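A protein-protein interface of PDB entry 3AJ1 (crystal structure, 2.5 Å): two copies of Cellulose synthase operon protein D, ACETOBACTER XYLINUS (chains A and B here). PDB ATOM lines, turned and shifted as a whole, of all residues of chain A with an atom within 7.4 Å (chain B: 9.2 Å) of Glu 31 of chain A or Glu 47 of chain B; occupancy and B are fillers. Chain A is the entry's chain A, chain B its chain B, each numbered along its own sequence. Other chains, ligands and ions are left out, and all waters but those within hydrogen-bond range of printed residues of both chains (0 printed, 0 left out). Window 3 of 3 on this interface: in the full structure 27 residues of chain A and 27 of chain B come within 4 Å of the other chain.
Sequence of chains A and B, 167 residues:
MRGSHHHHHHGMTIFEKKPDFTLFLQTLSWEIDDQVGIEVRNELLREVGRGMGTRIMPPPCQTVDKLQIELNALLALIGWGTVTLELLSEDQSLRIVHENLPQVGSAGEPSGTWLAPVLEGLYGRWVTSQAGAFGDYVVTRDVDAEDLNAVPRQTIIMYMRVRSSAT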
ATOM      1  N   LEU A  25     -11.074  23.114 -24.757  1.00  0.00           N
ATOM      2  CA  LEU A  25      -9.987  22.316 -25.313  1.00  0.00           C
ATOM      3  C   LEU A  25      -8.764  22.333 -24.415  1.00  0.00           C
ATOM      4  O   LEU A  25      -8.067  21.325 -24.277  1.00  0.00           O
ATOM      5  CB  LEU A  25      -9.644  22.779 -26.719  1.00  0.00           C
ATOM      6  CG  LEU A  25     -10.231  21.985 -27.884  1.00  0.00           C
ATOM      7  CD1 LEU A  25     -11.433  21.188 -27.479  1.00  0.00           C
ATOM      8  CD2 LEU A  25     -10.574  22.918 -29.013  1.00  0.00           C
ATOM      9  N   GLN A  26      -8.519  23.468 -23.778  1.00  0.00           N
ATOM     10  CA  GLN A  26      -7.381  23.587 -22.891  1.00  0.00           C
ATOM     11  C   GLN A  26      -7.481  22.602 -21.763  1.00  0.00           C
ATOM     12  O   GLN A  26      -6.516  21.914 -21.453  1.00  0.00           O
ATOM     13  CB  GLN A  26      -7.271  24.990 -22.336  1.00  0.00           C
ATOM     14  CG  GLN A  26      -6.486  25.928 -23.222  1.00  0.00           C
ATOM     15  CD  GLN A  26      -6.374  27.295 -22.597  1.00  0.00           C
ATOM     16  OE1 GLN A  26      -7.164  28.175 -22.902  1.00  0.00           O
ATOM     17  NE2 GLN A  26      -5.408  27.470 -21.689  1.00  0.00           N
ATOM     18  N   THR A  27      -8.655  22.511 -21.158  1.00  0.00           N
ATOM     19  CA  THR A  27      -8.797  21.638 -20.011  1.00  0.00           C
ATOM     20  C   THR A  27      -9.068  20.213 -20.480  1.00  0.00           C
ATOM     21  O   THR A  27      -8.757  19.264 -19.769  1.00  0.00           O
ATOM     22  CB  THR A  27      -9.870  22.129 -18.980  1.00  0.00           C
ATOM     23  OG1 THR A  27     -11.149  21.604 -19.337  1.00  0.00           O
ATOM     24  CG2 THR A  27      -9.952  23.638 -18.921  1.00  0.00           C
ATOM     25  N   LEU A  28      -9.642  20.064 -21.674  1.00  0.00           N
ATOM     26  CA  LEU A  28      -9.798  18.740 -22.271  1.00  0.00           C
ATOM     27  C   LEU A  28      -8.407  18.146 -22.551  1.00  0.00           C
ATOM     28  O   LEU A  28      -8.126  17.009 -22.178  1.00  0.00           O
ATOM     29  CB  LEU A  28     -10.653  18.782 -23.539  1.00  0.00           C
ATOM     30  CG  LEU A  28     -10.786  17.490 -24.374  1.00  0.00           C
ATOM     31  CD1 LEU A  28     -11.764  16.470 -23.779  1.00  0.00           C
ATOM     32  CD2 LEU A  28     -11.246  17.853 -25.740  1.00  0.00           C
ATOM     33  N   SER A  29      -7.522  18.926 -23.161  1.00  0.00           N
ATOM     34  CA  SER A  29      -6.174  18.417 -23.401  1.00  0.00           C
ATOM     35  C   SER A  29      -5.486  17.919 -22.111  1.00  0.00           C
ATOM     36  O   SER A  29      -4.790  16.892 -22.142  1.00  0.00           O
ATOM     37  CB  SER A  29      -5.312  19.432 -24.140  1.00  0.00           C
ATOM     38  OG  SER A  29      -4.877  20.446 -23.257  1.00  0.00           O
ATOM     39  N   TRP A  30      -5.686  18.618 -20.989  1.00  0.00           N
ATOM     40  CA  TRP A  30      -5.034  18.224 -19.731  1.00  0.00           C
ATOM     41  C   TRP A  30      -5.622  16.946 -19.158  1.00  0.00           C
ATOM     42  O   TRP A  30      -4.894  16.074 -18.689  1.00  0.00           O
ATOM     43  CB  TRP A  30      -5.113  19.335 -18.678  1.00  0.00           C
ATOM     44  CG  TRP A  30      -3.994  20.302 -18.744  1.00  0.00           C
ATOM     45  CD1 TRP A  30      -3.641  21.091 -19.812  1.00  0.00           C
ATOM     46  CD2 TRP A  30      -3.070  20.611 -17.695  1.00  0.00           C
ATOM     47  NE1 TRP A  30      -2.546  21.862 -19.491  1.00  0.00           N
ATOM     48  CE2 TRP A  30      -2.177  21.590 -18.197  1.00  0.00           C
ATOM     49  CE3 TRP A  30      -2.901  20.148 -16.381  1.00  0.00           C
ATOM     50  CZ2 TRP A  30      -1.141  22.114 -17.431  1.00  0.00           C
ATOM     51  CZ3 TRP A  30      -1.864  20.675 -15.618  1.00  0.00           C
ATOM     52  CH2 TRP A  30      -1.001  21.647 -16.149  1.00  0.00           C
ATOM     53  N   GLU A  31      -6.945  16.852 -19.187  1.00  0.00           N
ATOM     54  CA  GLU A  31      -7.618  15.682 -18.660  1.00  0.00           C
ATOM     55  C   GLU A  31      -7.296  14.414 -19.466  1.00  0.00           C
ATOM     56  O   GLU A  31      -7.006  13.365 -18.875  1.00  0.00           O
ATOM     57  CB  GLU A  31      -9.129  15.915 -18.561  1.00  0.00           C
ATOM     58  CG  GLU A  31      -9.864  14.874 -17.716  1.00  0.00           C
ATOM     59  CD  GLU A  31      -9.226  14.640 -16.336  1.00  0.00           C
ATOM     60  OE1 GLU A  31      -8.585  15.578 -15.791  1.00  0.00           O
ATOM     61  OE2 GLU A  31      -9.374  13.509 -15.795  1.00  0.00           O
ATOM     62  N   ILE A  32      -7.327  14.521 -20.798  1.00  0.00           N
ATOM     63  CA  ILE A  32      -7.053  13.373 -21.666  1.00  0.00           C
ATOM     64  C   ILE A  32      -5.610  12.890 -21.486  1.00  0.00           C
ATOM     65  O   ILE A  32      -5.377  11.677 -21.349  1.00  0.00           O
ATOM     66  CB  ILE A  32      -7.356  13.655 -23.175  1.00  0.00           C
ATOM     67  CG1 ILE A  32      -8.867  13.724 -23.423  1.00  0.00           C
ATOM     68  CG2 ILE A  32      -6.733  12.581 -24.060  1.00  0.00           C
ATOM     69  CD1 ILE A  32      -9.262  14.025 -24.884  1.00  0.00           C
ATOM     70  N   ASP A  33      -4.661  13.838 -21.476  1.00  0.00           N
ATOM     71  CA  ASP A  33      -3.247  13.504 -21.308  1.00  0.00           C
ATOM     72  C   ASP A  33      -3.012  12.722 -20.035  1.00  0.00           C
ATOM     73  O   ASP A  33      -2.253  11.748 -20.030  1.00  0.00           O
ATOM     74  CB  ASP A  33      -2.368  14.746 -21.284  1.00  0.00           C
ATOM     75  CG  ASP A  33      -2.083  15.281 -22.658  1.00  0.00           C
ATOM     76  OD1 ASP A  33      -2.704  14.777 -23.628  1.00  0.00           O
ATOM     77  OD2 ASP A  33      -1.235  16.206 -22.767  1.00  0.00           O
ATOM     78  N   ASP A  34      -3.673  13.137 -18.963  1.00  0.00           N
ATOM     79  CA  ASP A  34      -3.450  12.534 -17.667  1.00  0.00           C
ATOM     80  C   ASP A  34      -4.051  11.134 -17.528  1.00  0.00           C
ATOM     81  O   ASP A  34      -3.526  10.319 -16.790  1.00  0.00           O
ATOM     82  CB  ASP A  34      -3.971  13.448 -16.553  1.00  0.00           C
ATOM     83  CG  ASP A  34      -3.714  12.877 -15.165  1.00  0.00           C
ATOM     84  OD1 ASP A  34      -4.703  12.685 -14.415  1.00  0.00           O
ATOM     85  OD2 ASP A  34      -2.530  12.590 -14.841  1.00  0.00           O
ATOM     86  N   GLN A  35      -5.153  10.864 -18.218  1.00  0.00           N
ATOM     87  CA  GLN A  35      -5.802   9.552 -18.134  1.00  0.00           C
ATOM     88  C   GLN A  35      -5.162   8.477 -19.017  1.00  0.00           C
ATOM     89  O   GLN A  35      -5.101   7.321 -18.615  1.00  0.00           O
ATOM     90  CB  GLN A  35      -7.285   9.648 -18.469  1.00  0.00           C
ATOM     91  CG  GLN A  35      -8.085  10.458 -17.475  1.00  0.00           C
ATOM     92  CD  GLN A  35      -9.555  10.112 -17.498  1.00  0.00           C
ATOM     93  OE1 GLN A  35      -9.952   9.058 -17.998  1.00  0.00           O
ATOM     94  NE2 GLN A  35     -10.379  10.999 -16.943  1.00  0.00           N
ATOM     95  N   VAL A  36      -4.679   8.865 -20.199  1.00  0.00           N
ATOM     96  CA  VAL A  36      -4.275   7.898 -21.218  1.00  0.00           C
ATOM     97  C   VAL A  36      -2.852   8.015 -21.731  1.00  0.00           C
ATOM     98  O   VAL A  36      -2.371   7.114 -22.416  1.00  0.00           O
ATOM     99  CB  VAL A  36      -5.263   7.848 -22.423  1.00  0.00           C
ATOM    100  CG1 VAL A  36      -6.694   7.615 -21.941  1.00  0.00           C
ATOM    101  CG2 VAL A  36      -5.158   9.106 -23.300  1.00  0.00           C
ATOM    102  N   GLY A  37      -2.176   9.111 -21.430  1.00  0.00           N
ATOM    103  CA  GLY A  37      -0.795   9.281 -21.878  1.00  0.00           C
ATOM    104  C   GLY A  37      -0.625   9.757 -23.311  1.00  0.00           C
ATOM    105  O   GLY A  37      -1.532   9.638 -24.148  1.00  0.00           O
ATOM    106  N   GLU B  39     -21.304   6.173 -20.138  1.00  0.00           N
ATOM    107  CA  GLU B  39     -20.958   6.420 -18.746  1.00  0.00           C
ATOM    108  C   GLU B  39     -19.575   7.013 -18.583  1.00  0.00           C
ATOM    109  O   GLU B  39     -19.361   7.881 -17.738  1.00  0.00           O
ATOM    110  CB  GLU B  39     -21.038   5.143 -17.922  1.00  0.00           C
ATOM    111  CG  GLU B  39     -21.855   5.312 -16.654  1.00  0.00           C
ATOM    112  CD  GLU B  39     -23.336   5.472 -16.948  1.00  0.00           C
ATOM    113  OE1 GLU B  39     -23.931   4.559 -17.571  1.00  0.00           O
ATOM    114  OE2 GLU B  39     -23.909   6.512 -16.565  1.00  0.00           O
ATOM    115  N   VAL B  40     -18.641   6.545 -19.393  1.00  0.00           N
ATOM    116  CA  VAL B  40     -17.247   6.928 -19.261  1.00  0.00           C
ATOM    117  C   VAL B  40     -16.997   8.261 -19.962  1.00  0.00           C
ATOM    118  O   VAL B  40     -16.225   9.075 -19.493  1.00  0.00           O
ATOM    119  CB  VAL B  40     -16.330   5.792 -19.779  1.00  0.00           C
ATOM    120  CG1 VAL B  40     -14.879   6.227 -19.851  1.00  0.00           C
ATOM    121  CG2 VAL B  40     -16.490   4.576 -18.887  1.00  0.00           C
ATOM    122  N   ARG B  41     -17.668   8.470 -21.085  1.00  0.00           N
ATOM    123  CA  ARG B  41     -17.687   9.764 -21.739  1.00  0.00           C
ATOM    124  C   ARG B  41     -18.180  10.837 -20.781  1.00  0.00           C
ATOM    125  O   ARG B  41     -17.609  11.927 -20.743  1.00  0.00           O
ATOM    126  CB  ARG B  41     -18.613   9.757 -22.936  1.00  0.00           C
ATOM    127  CG  ARG B  41     -18.834  11.157 -23.477  1.00  0.00           C
ATOM    128  CD  ARG B  41     -19.911  11.163 -24.485  1.00  0.00           C
ATOM    129  NE  ARG B  41     -21.220  11.125 -23.858  1.00  0.00           N
ATOM    130  CZ  ARG B  41     -22.344  10.731 -24.443  1.00  0.00           C
ATOM    131  NH1 ARG B  41     -22.350  10.289 -25.681  1.00  0.00           N
ATOM    132  NH2 ARG B  41     -23.472  10.762 -23.760  1.00  0.00           N
ATOM    133  N   ASN B  42     -19.248  10.521 -20.040  1.00  0.00           N
ATOM    134  CA  ASN B  42     -19.853  11.446 -19.098  1.00  0.00           C
ATOM    135  C   ASN B  42     -18.942  11.758 -17.915  1.00  0.00           C
ATOM    136  O   ASN B  42     -18.908  12.897 -17.456  1.00  0.00           O
ATOM    137  CB  ASN B  42     -21.201  10.935 -18.597  1.00  0.00           C
ATOM    138  CG  ASN B  42     -22.324  11.097 -19.621  1.00  0.00           C
ATOM    139  OD1 ASN B  42     -22.159  11.710 -20.679  1.00  0.00           O
ATOM    140  ND2 ASN B  42     -23.477  10.522 -19.304  1.00  0.00           N
ATOM    141  N   GLU B  43     -18.186  10.776 -17.429  1.00  0.00           N
ATOM    142  CA  GLU B  43     -17.300  11.076 -16.314  1.00  0.00           C
ATOM    143  C   GLU B  43     -16.166  11.955 -16.758  1.00  0.00           C
ATOM    144  O   GLU B  43     -15.812  12.898 -16.050  1.00  0.00           O
ATOM    145  CB  GLU B  43     -16.767   9.836 -15.590  1.00  0.00           C
ATOM    146  CG  GLU B  43     -17.420   9.594 -14.214  1.00  0.00           C
ATOM    147  CD  GLU B  43     -17.593  10.866 -13.348  1.00  0.00           C
ATOM    148  OE1 GLU B  43     -16.596  11.614 -13.117  1.00  0.00           O
ATOM    149  OE2 GLU B  43     -18.749  11.104 -12.903  1.00  0.00           O
ATOM    150  N   LEU B  44     -15.598  11.642 -17.920  1.00  0.00           N
ATOM    151  CA  LEU B  44     -14.517  12.432 -18.490  1.00  0.00           C
ATOM    152  C   LEU B  44     -14.968  13.894 -18.629  1.00  0.00           C
ATOM    153  O   LEU B  44     -14.331  14.785 -18.079  1.00  0.00           O
ATOM    154  CB  LEU B  44     -14.098  11.868 -19.847  1.00  0.00           C
ATOM    155  CG  LEU B  44     -13.072  12.643 -20.676  1.00  0.00           C
ATOM    156  CD1 LEU B  44     -11.747  12.753 -19.971  1.00  0.00           C
ATOM    157  CD2 LEU B  44     -12.907  11.953 -21.998  1.00  0.00           C
ATOM    158  N   LEU B  45     -16.092  14.104 -19.325  1.00  0.00           N
ATOM    159  CA  LEU B  45     -16.688  15.423 -19.494  1.00  0.00           C
ATOM    160  C   LEU B  45     -16.974  16.180 -18.173  1.00  0.00           C
ATOM    161  O   LEU B  45     -16.696  17.376 -18.088  1.00  0.00           O
ATOM    162  CB  LEU B  45     -17.918  15.358 -20.409  1.00  0.00           C
ATOM    163  CG  LEU B  45     -17.673  15.042 -21.892  1.00  0.00           C
ATOM    164  CD1 LEU B  45     -18.943  15.144 -22.673  1.00  0.00           C
ATOM    165  CD2 LEU B  45     -16.599  15.924 -22.543  1.00  0.00           C
ATOM    166  N   ARG B  46     -17.494  15.497 -17.150  1.00  0.00           N
ATOM    167  CA  ARG B  46     -17.659  16.110 -15.821  1.00  0.00           C
ATOM    168  C   ARG B  46     -16.338  16.598 -15.270  1.00  0.00           C
ATOM    169  O   ARG B  46     -16.258  17.707 -14.727  1.00  0.00           O
ATOM    170  CB  ARG B  46     -18.268  15.151 -14.818  1.00  0.00           C
ATOM    171  CG  ARG B  46     -19.720  14.930 -15.045  1.00  0.00           C
ATOM    172  CD  ARG B  46     -20.343  14.119 -13.960  1.00  0.00           C
ATOM    173  NE  ARG B  46     -21.500  13.424 -14.499  1.00  0.00           N
ATOM    174  CZ  ARG B  46     -21.516  12.132 -14.809  1.00  0.00           C
ATOM    175  NH1 ARG B  46     -20.431  11.388 -14.601  1.00  0.00           N
ATOM    176  NH2 ARG B  46     -22.622  11.580 -15.309  1.00  0.00           N
ATOM    177  N   GLU B  47     -15.313  15.766 -15.413  1.00  0.00           N
ATOM    178  CA  GLU B  47     -13.955  16.079 -14.985  1.00  0.00           C
ATOM    179  C   GLU B  47     -13.392  17.303 -15.700  1.00  0.00           C
ATOM    180  O   GLU B  47     -12.764  18.139 -15.071  1.00  0.00           O
ATOM    181  CB  GLU B  47     -13.041  14.870 -15.223  1.00  0.00           C
ATOM    182  CG  GLU B  47     -12.005  14.671 -14.162  1.00  0.00           C
ATOM    183  CD  GLU B  47     -12.603  14.709 -12.762  1.00  0.00           C
ATOM    184  OE1 GLU B  47     -13.422  13.824 -12.440  1.00  0.00           O
ATOM    185  OE2 GLU B  47     -12.258  15.635 -11.989  1.00  0.00           O
ATOM    186  N   VAL B  48     -13.605  17.392 -17.010  1.00  0.00           N
ATOM    187  CA  VAL B  48     -13.202  18.542 -17.811  1.00  0.00           C
ATOM    188  C   VAL B  48     -13.918  19.820 -17.323  1.00  0.00           C
ATOM    189  O   VAL B  48     -13.302  20.888 -17.217  1.00  0.00           O
ATOM    190  CB  VAL B  48     -13.488  18.302 -19.313  1.00  0.00           C
ATOM    191  CG1 VAL B  48     -13.292  19.584 -20.132  1.00  0.00           C
ATOM    192  CG2 VAL B  48     -12.620  17.164 -19.851  1.00  0.00           C
ATOM    193  N   GLY B  49     -15.212  19.693 -17.036  1.00  0.00           N
ATOM    194  CA  GLY B  49     -15.982  20.760 -16.423  1.00  0.00           C
ATOM    195  C   GLY B  49     -15.400  21.232 -15.101  1.00  0.00           C
ATOM    196  O   GLY B  49     -15.321  22.436 -14.858  1.00  0.00           O
ATOM    197  N   ARG B  50     -15.008  20.295 -14.239  1.00  0.00           N
ATOM    198  CA  ARG B  50     -14.385  20.643 -12.968  1.00  0.00           C
ATOM    199  C   ARG B  50     -13.130  21.449 -13.249  1.00  0.00           C
ATOM    200  O   ARG B  50     -12.860  22.463 -12.584  1.00  0.00           O
ATOM    201  CB  ARG B  50     -14.022  19.397 -12.163  1.00  0.00           C
ATOM    202  CG  ARG B  50     -15.185  18.738 -11.469  1.00  0.00           C
ATOM    203  CD  ARG B  50     -14.888  17.271 -11.255  1.00  0.00           C
ATOM    204  NE  ARG B  50     -15.986  16.531 -10.637  1.00  0.00           N
ATOM    205  CZ  ARG B  50     -16.309  15.270 -10.931  1.00  0.00           C
ATOM    206  NH1 ARG B  50     -15.641  14.594 -11.859  1.00  0.00           N
ATOM    207  NH2 ARG B  50     -17.318  14.685 -10.301  1.00  0.00           N
ATOM    208  N   GLY B  51     -12.380  20.988 -14.250  1.00  0.00           N
ATOM    209  CA  GLY B  51     -11.153  21.630 -14.667  1.00  0.00           C
ATOM    210  C   GLY B  51     -11.403  23.060 -15.101  1.00  0.00           C
ATOM    211  O   GLY B  51     -10.670  23.961 -14.702  1.00  0.00           O
ATOM    212  N   MET B  52     -12.438  23.269 -15.910  1.00  0.00           N
ATOM    213  CA  MET B  52     -12.752  24.606 -16.419  1.00  0.00           C
ATOM    214  C   MET B  52     -13.044  25.532 -15.240  1.00  0.00           C
ATOM    215  O   MET B  52     -12.650  26.696 -15.240  1.00  0.00           O
ATOM    216  CB  MET B  52     -13.945  24.579 -17.371  1.00  0.00           C
ATOM    217  CG  MET B  52     -13.653  23.974 -18.707  1.00  0.00           C
ATOM    218  SD  MET B  52     -15.253  23.915 -19.793  1.00  0.00           S
ATOM    219  CE  MET B  52     -15.269  25.711 -20.580  1.00  0.00           C
ATOM    220  N   GLY B  53     -13.710  24.960 -14.238  1.00  0.00           N
ATOM    221  CA  GLY B  53     -14.070  25.641 -13.007  1.00  0.00           C
ATOM    222  C   GLY B  53     -12.912  25.979 -12.073  1.00  0.00           C
ATOM    223  O   GLY B  53     -13.129  26.647 -11.078  1.00  0.00           O
ATOM    224  N   THR B  54     -11.695  25.535 -12.382  1.00  0.00           N
ATOM    225  CA  THR B  54     -10.517  25.988 -11.631  1.00  0.00           C
ATOM    226  C   THR B  54      -9.690  27.034 -12.402  1.00  0.00           C
ATOM    227  O   THR B  54      -8.617  27.420 -11.952  1.00  0.00           O
ATOM    228  CB  THR B  54      -9.573  24.820 -11.251  1.00  0.00           C
ATOM    229  OG1 THR B  54      -8.904  24.352 -12.425  1.00  0.00           O
ATOM    230  CG2 THR B  54     -10.349  23.679 -10.640  1.00  0.00           C
ATOM    231  N   ARG B  55     -10.191  27.476 -13.554  1.00  0.00           N
ATOM    232  CA  ARG B  55      -9.494  28.443 -14.387  1.00  0.00           C
ATOM    233  C   ARG B  55     -10.250  29.760 -14.485  1.00  0.00           C
ATOM    234  O   ARG B  55      -9.641  30.836 -14.548  1.00  0.00           O
ATOM    235  CB  ARG B  55      -9.297  27.898 -15.803  1.00  0.00           C
ATOM    236  CG  ARG B  55      -8.827  26.469 -15.874  1.00  0.00           C
ATOM    237  CD  ARG B  55      -7.650  26.402 -16.763  1.00  0.00           C
ATOM    238  NE  ARG B  55      -7.249  25.036 -17.083  1.00  0.00           N
ATOM    239  CZ  ARG B  55      -6.412  24.733 -18.070  1.00  0.00           C
ATOM    240  NH1 ARG B  55      -5.902  25.700 -18.826  1.00  0.00           N
ATOM    241  NH2 ARG B  55      -6.086  23.471 -18.298  1.00  0.00           N
ATOM    242  N   PRO B 117     -22.655  17.148 -19.654  1.00  0.00           N
ATOM    243  CA  PRO B 117     -21.948  16.763 -18.430  1.00  0.00           C
ATOM    244  C   PRO B 117     -20.859  17.740 -17.998  1.00  0.00           C
ATOM    245  O   PRO B 117     -20.550  17.798 -16.815  1.00  0.00           O
ATOM    246  CB  PRO B 117     -21.317  15.415 -18.798  1.00  0.00           C
ATOM    247  CG  PRO B 117     -22.163  14.891 -19.859  1.00  0.00           C
ATOM    248  CD  PRO B 117     -22.654  16.050 -20.644  1.00  0.00           C
ATOM    249  N   VAL B 118     -20.263  18.470 -18.941  1.00  0.00           N
ATOM    250  CA  VAL B 118     -19.302  19.539 -18.609  1.00  0.00           C
ATOM    251  C   VAL B 118     -19.915  20.544 -17.622  1.00  0.00           C
ATOM    252  O   VAL B 118     -19.222  21.050 -16.750  1.00  0.00           O
ATOM    253  CB  VAL B 118     -18.812  20.306 -19.858  1.00  0.00           C
ATOM    254  CG1 VAL B 118     -17.698  21.242 -19.497  1.00  0.00           C
ATOM    255  CG2 VAL B 118     -18.332  19.344 -20.918  1.00  0.00           C
ATOM    256  N   LEU B 119     -21.214  20.812 -17.764  1.00  0.00           N
ATOM    257  CA  LEU B 119     -21.919  21.741 -16.870  1.00  0.00           C
ATOM    258  C   LEU B 119     -22.022  21.219 -15.448  1.00  0.00           C
ATOM    259  O   LEU B 119     -21.856  21.986 -14.499  1.00  0.00           O
ATOM    260  CB  LEU B 119     -23.294  22.094 -17.427  1.00  0.00           C
ATOM    261  CG  LEU B 119     -23.473  23.345 -18.310  1.00  0.00           C
ATOM    262  CD1 LEU B 119     -22.223  23.807 -19.051  1.00  0.00           C
ATOM    263  CD2 LEU B 119     -24.593  23.112 -19.257  1.00  0.00           C
ATOM    264  N   GLU B 120     -22.247  19.911 -15.299  1.00  0.00           N
ATOM    265  CA  GLU B 120     -22.368  19.289 -13.987  1.00  0.00           C
ATOM    266  C   GLU B 120     -21.100  19.508 -13.205  1.00  0.00           C
ATOM    267  O   GLU B 120     -21.144  19.855 -12.025  1.00  0.00           O
ATOM    268  CB  GLU B 120     -22.672  17.800 -14.110  1.00  0.00           C
ATOM    269  CG  GLU B 120     -24.038  17.497 -14.711  1.00  0.00           C
ATOM    270  CD  GLU B 120     -24.289  16.011 -14.901  1.00  0.00           C
ATOM    271  OE1 GLU B 120     -23.454  15.334 -15.524  1.00  0.00           O
ATOM    272  OE2 GLU B 120     -25.335  15.514 -14.443  1.00  0.00           O
ATOM    273  N   GLY B 121     -19.969  19.335 -13.883  1.00  0.00           N
ATOM    274  CA  GLY B 121     -18.668  19.539 -13.293  1.00  0.00           C
ATOM    275  C   GLY B 121     -18.412  21.006 -13.041  1.00  0.00           C
ATOM    276  O   GLY B 121     -17.915  21.361 -11.979  1.00  0.00           O
ATOM    277  N   LEU B 122     -18.766  21.857 -14.006  1.00  0.00           N
ATOM    278  CA  LEU B 122     -18.556  23.303 -13.889  1.00  0.00           C
ATOM    279  C   LEU B 122     -19.390  23.948 -12.768  1.00  0.00           C
ATOM    280  O   LEU B 122     -18.832  24.589 -11.870  1.00  0.00           O
ATOM    281  CB  LEU B 122     -18.822  24.013 -15.216  1.00  0.00           C
ATOM    282  CG  LEU B 122     -18.500  25.512 -15.315  1.00  0.00           C
ATOM    283  CD1 LEU B 122     -17.020  25.793 -15.208  1.00  0.00           C
ATOM    284  CD2 LEU B 122     -19.018  26.036 -16.641  1.00  0.00           C
ATOM    285  N   ARG B 125     -18.253  22.987  -9.516  1.00  0.00           N
ATOM    286  CA  ARG B 125     -17.135  23.786  -9.002  1.00  0.00           C
ATOM    287  C   ARG B 125     -17.580  25.224  -8.611  1.00  0.00           C
ATOM    288  O   ARG B 125     -17.194  25.730  -7.566  1.00  0.00           O
ATOM    289  CB  ARG B 125     -15.978  23.785 -10.010  1.00  0.00           C
ATOM    290  CG  ARG B 125     -14.574  24.073  -9.440  1.00  0.00           C
ATOM    291  CD  ARG B 125     -14.050  22.973  -8.499  1.00  0.00           C
ATOM    292  NE  ARG B 125     -13.250  21.944  -9.172  1.00  0.00           N
ATOM    293  CZ  ARG B 125     -12.006  21.594  -8.821  1.00  0.00           C
ATOM    294  NH1 ARG B 125     -11.393  22.193  -7.799  1.00  0.00           N
ATOM    295  NH2 ARG B 125     -11.363  20.644  -9.499  1.00  0.00           N
ATOM    296  N   THR B 167     -19.305  10.716  -6.342  1.00  0.00           N
ATOM    297  CA  THR B 167     -18.096  11.557  -6.443  1.00  0.00           C
ATOM    298  C   THR B 167     -16.970  10.883  -7.251  1.00  0.00           C
ATOM    299  O   THR B 167     -16.488   9.795  -6.917  1.00  0.00           O
ATOM    300  CB  THR B 167     -17.587  12.053  -5.050  1.00  0.00           C
ATOM    301  OG1 THR B 167     -18.468  13.081  -4.565  1.00  0.00           O
ATOM    302  CG2 THR B 167     -16.169  12.626  -5.145  1.00  0.00           C
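The backbone carbonyl oxygen (O) of Val 48 of chain B lies close to the side-chain hydroxyl (OG1) of Thr 27 of chain A (3.1 Å).
The side-chain amide nitrogen of Gln 26 of chain A lies close to the guanidinium group of Arg 55 of chain B.
The side-chain carboxylate (OE2) of Glu 31 of chain A is in hydrogen-bond range of the side-chain amide nitrogen (NE2) of Gln 35 of chain A, at 2.9 Å.
OG of Ser 29 of chain A is in hydrogen-bond range of O of Gln 26 of chain A.
OE1 of Glu 47 of chain B lies within salt-bridge range of NH1 of Arg 50 of chain B, 2.4 Å away.
Among the printed residues, pairs that only touch across the chains: Thr 27 of chain A with Met 52 of chain B (3.5 Å), Thr 27 of chain A with Arg 55 of chain B (3.6 Å), Leu 28 of chain A with Val 48 of chain B (3.99 Å), Trp 30 of chain A with Arg 55 of chain B (3.7 Å), Glu 31 of chain A with Leu 44 of chain B (3.6 Å), Glu 31 of chain A with Glu 47 of chain B (3.3 Å), Glu 31 of chain A with Val 48 of chain B (3.9 Å) and Gln 35 of chain A with Leu 44 of chain B (3.8 Å).
Of the printed residues of chain B, Gln 26 of chain A touches Arg 55 (3.4 Å).
Of the printed residues of chain B, Thr 27 of chain A touches Val 48, Met 52 and Arg 55.
Gly 37 of chain A touches none of the printed residues of chain B.
Of the printed residues of chain A, Glu 47 of chain B touches Glu 31 (3.3 Å).
Arg 125 of chain B touches none of the printed residues of chain A.
The nearest residue of chain A that does not touch Glu 47 of chain B is Gln 35 of chain A (4.9 Å).
Printed residues of chain B that touch a printed residue of chain A: Leu 44, Glu 47, Val 48, Met 52 and Arg 55.
Among the printed residues, 10 pairs touch across the chains.
Among the printed residues, no Asp or Glu carboxylate lies within 4 Å of a Lys or Arg side-chain nitrogen of the other chain.
No position is printed for both chains.
Of the 10 pairs that touch across the chains among the printed residues, none has its exchanged pair printed and touching as well.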
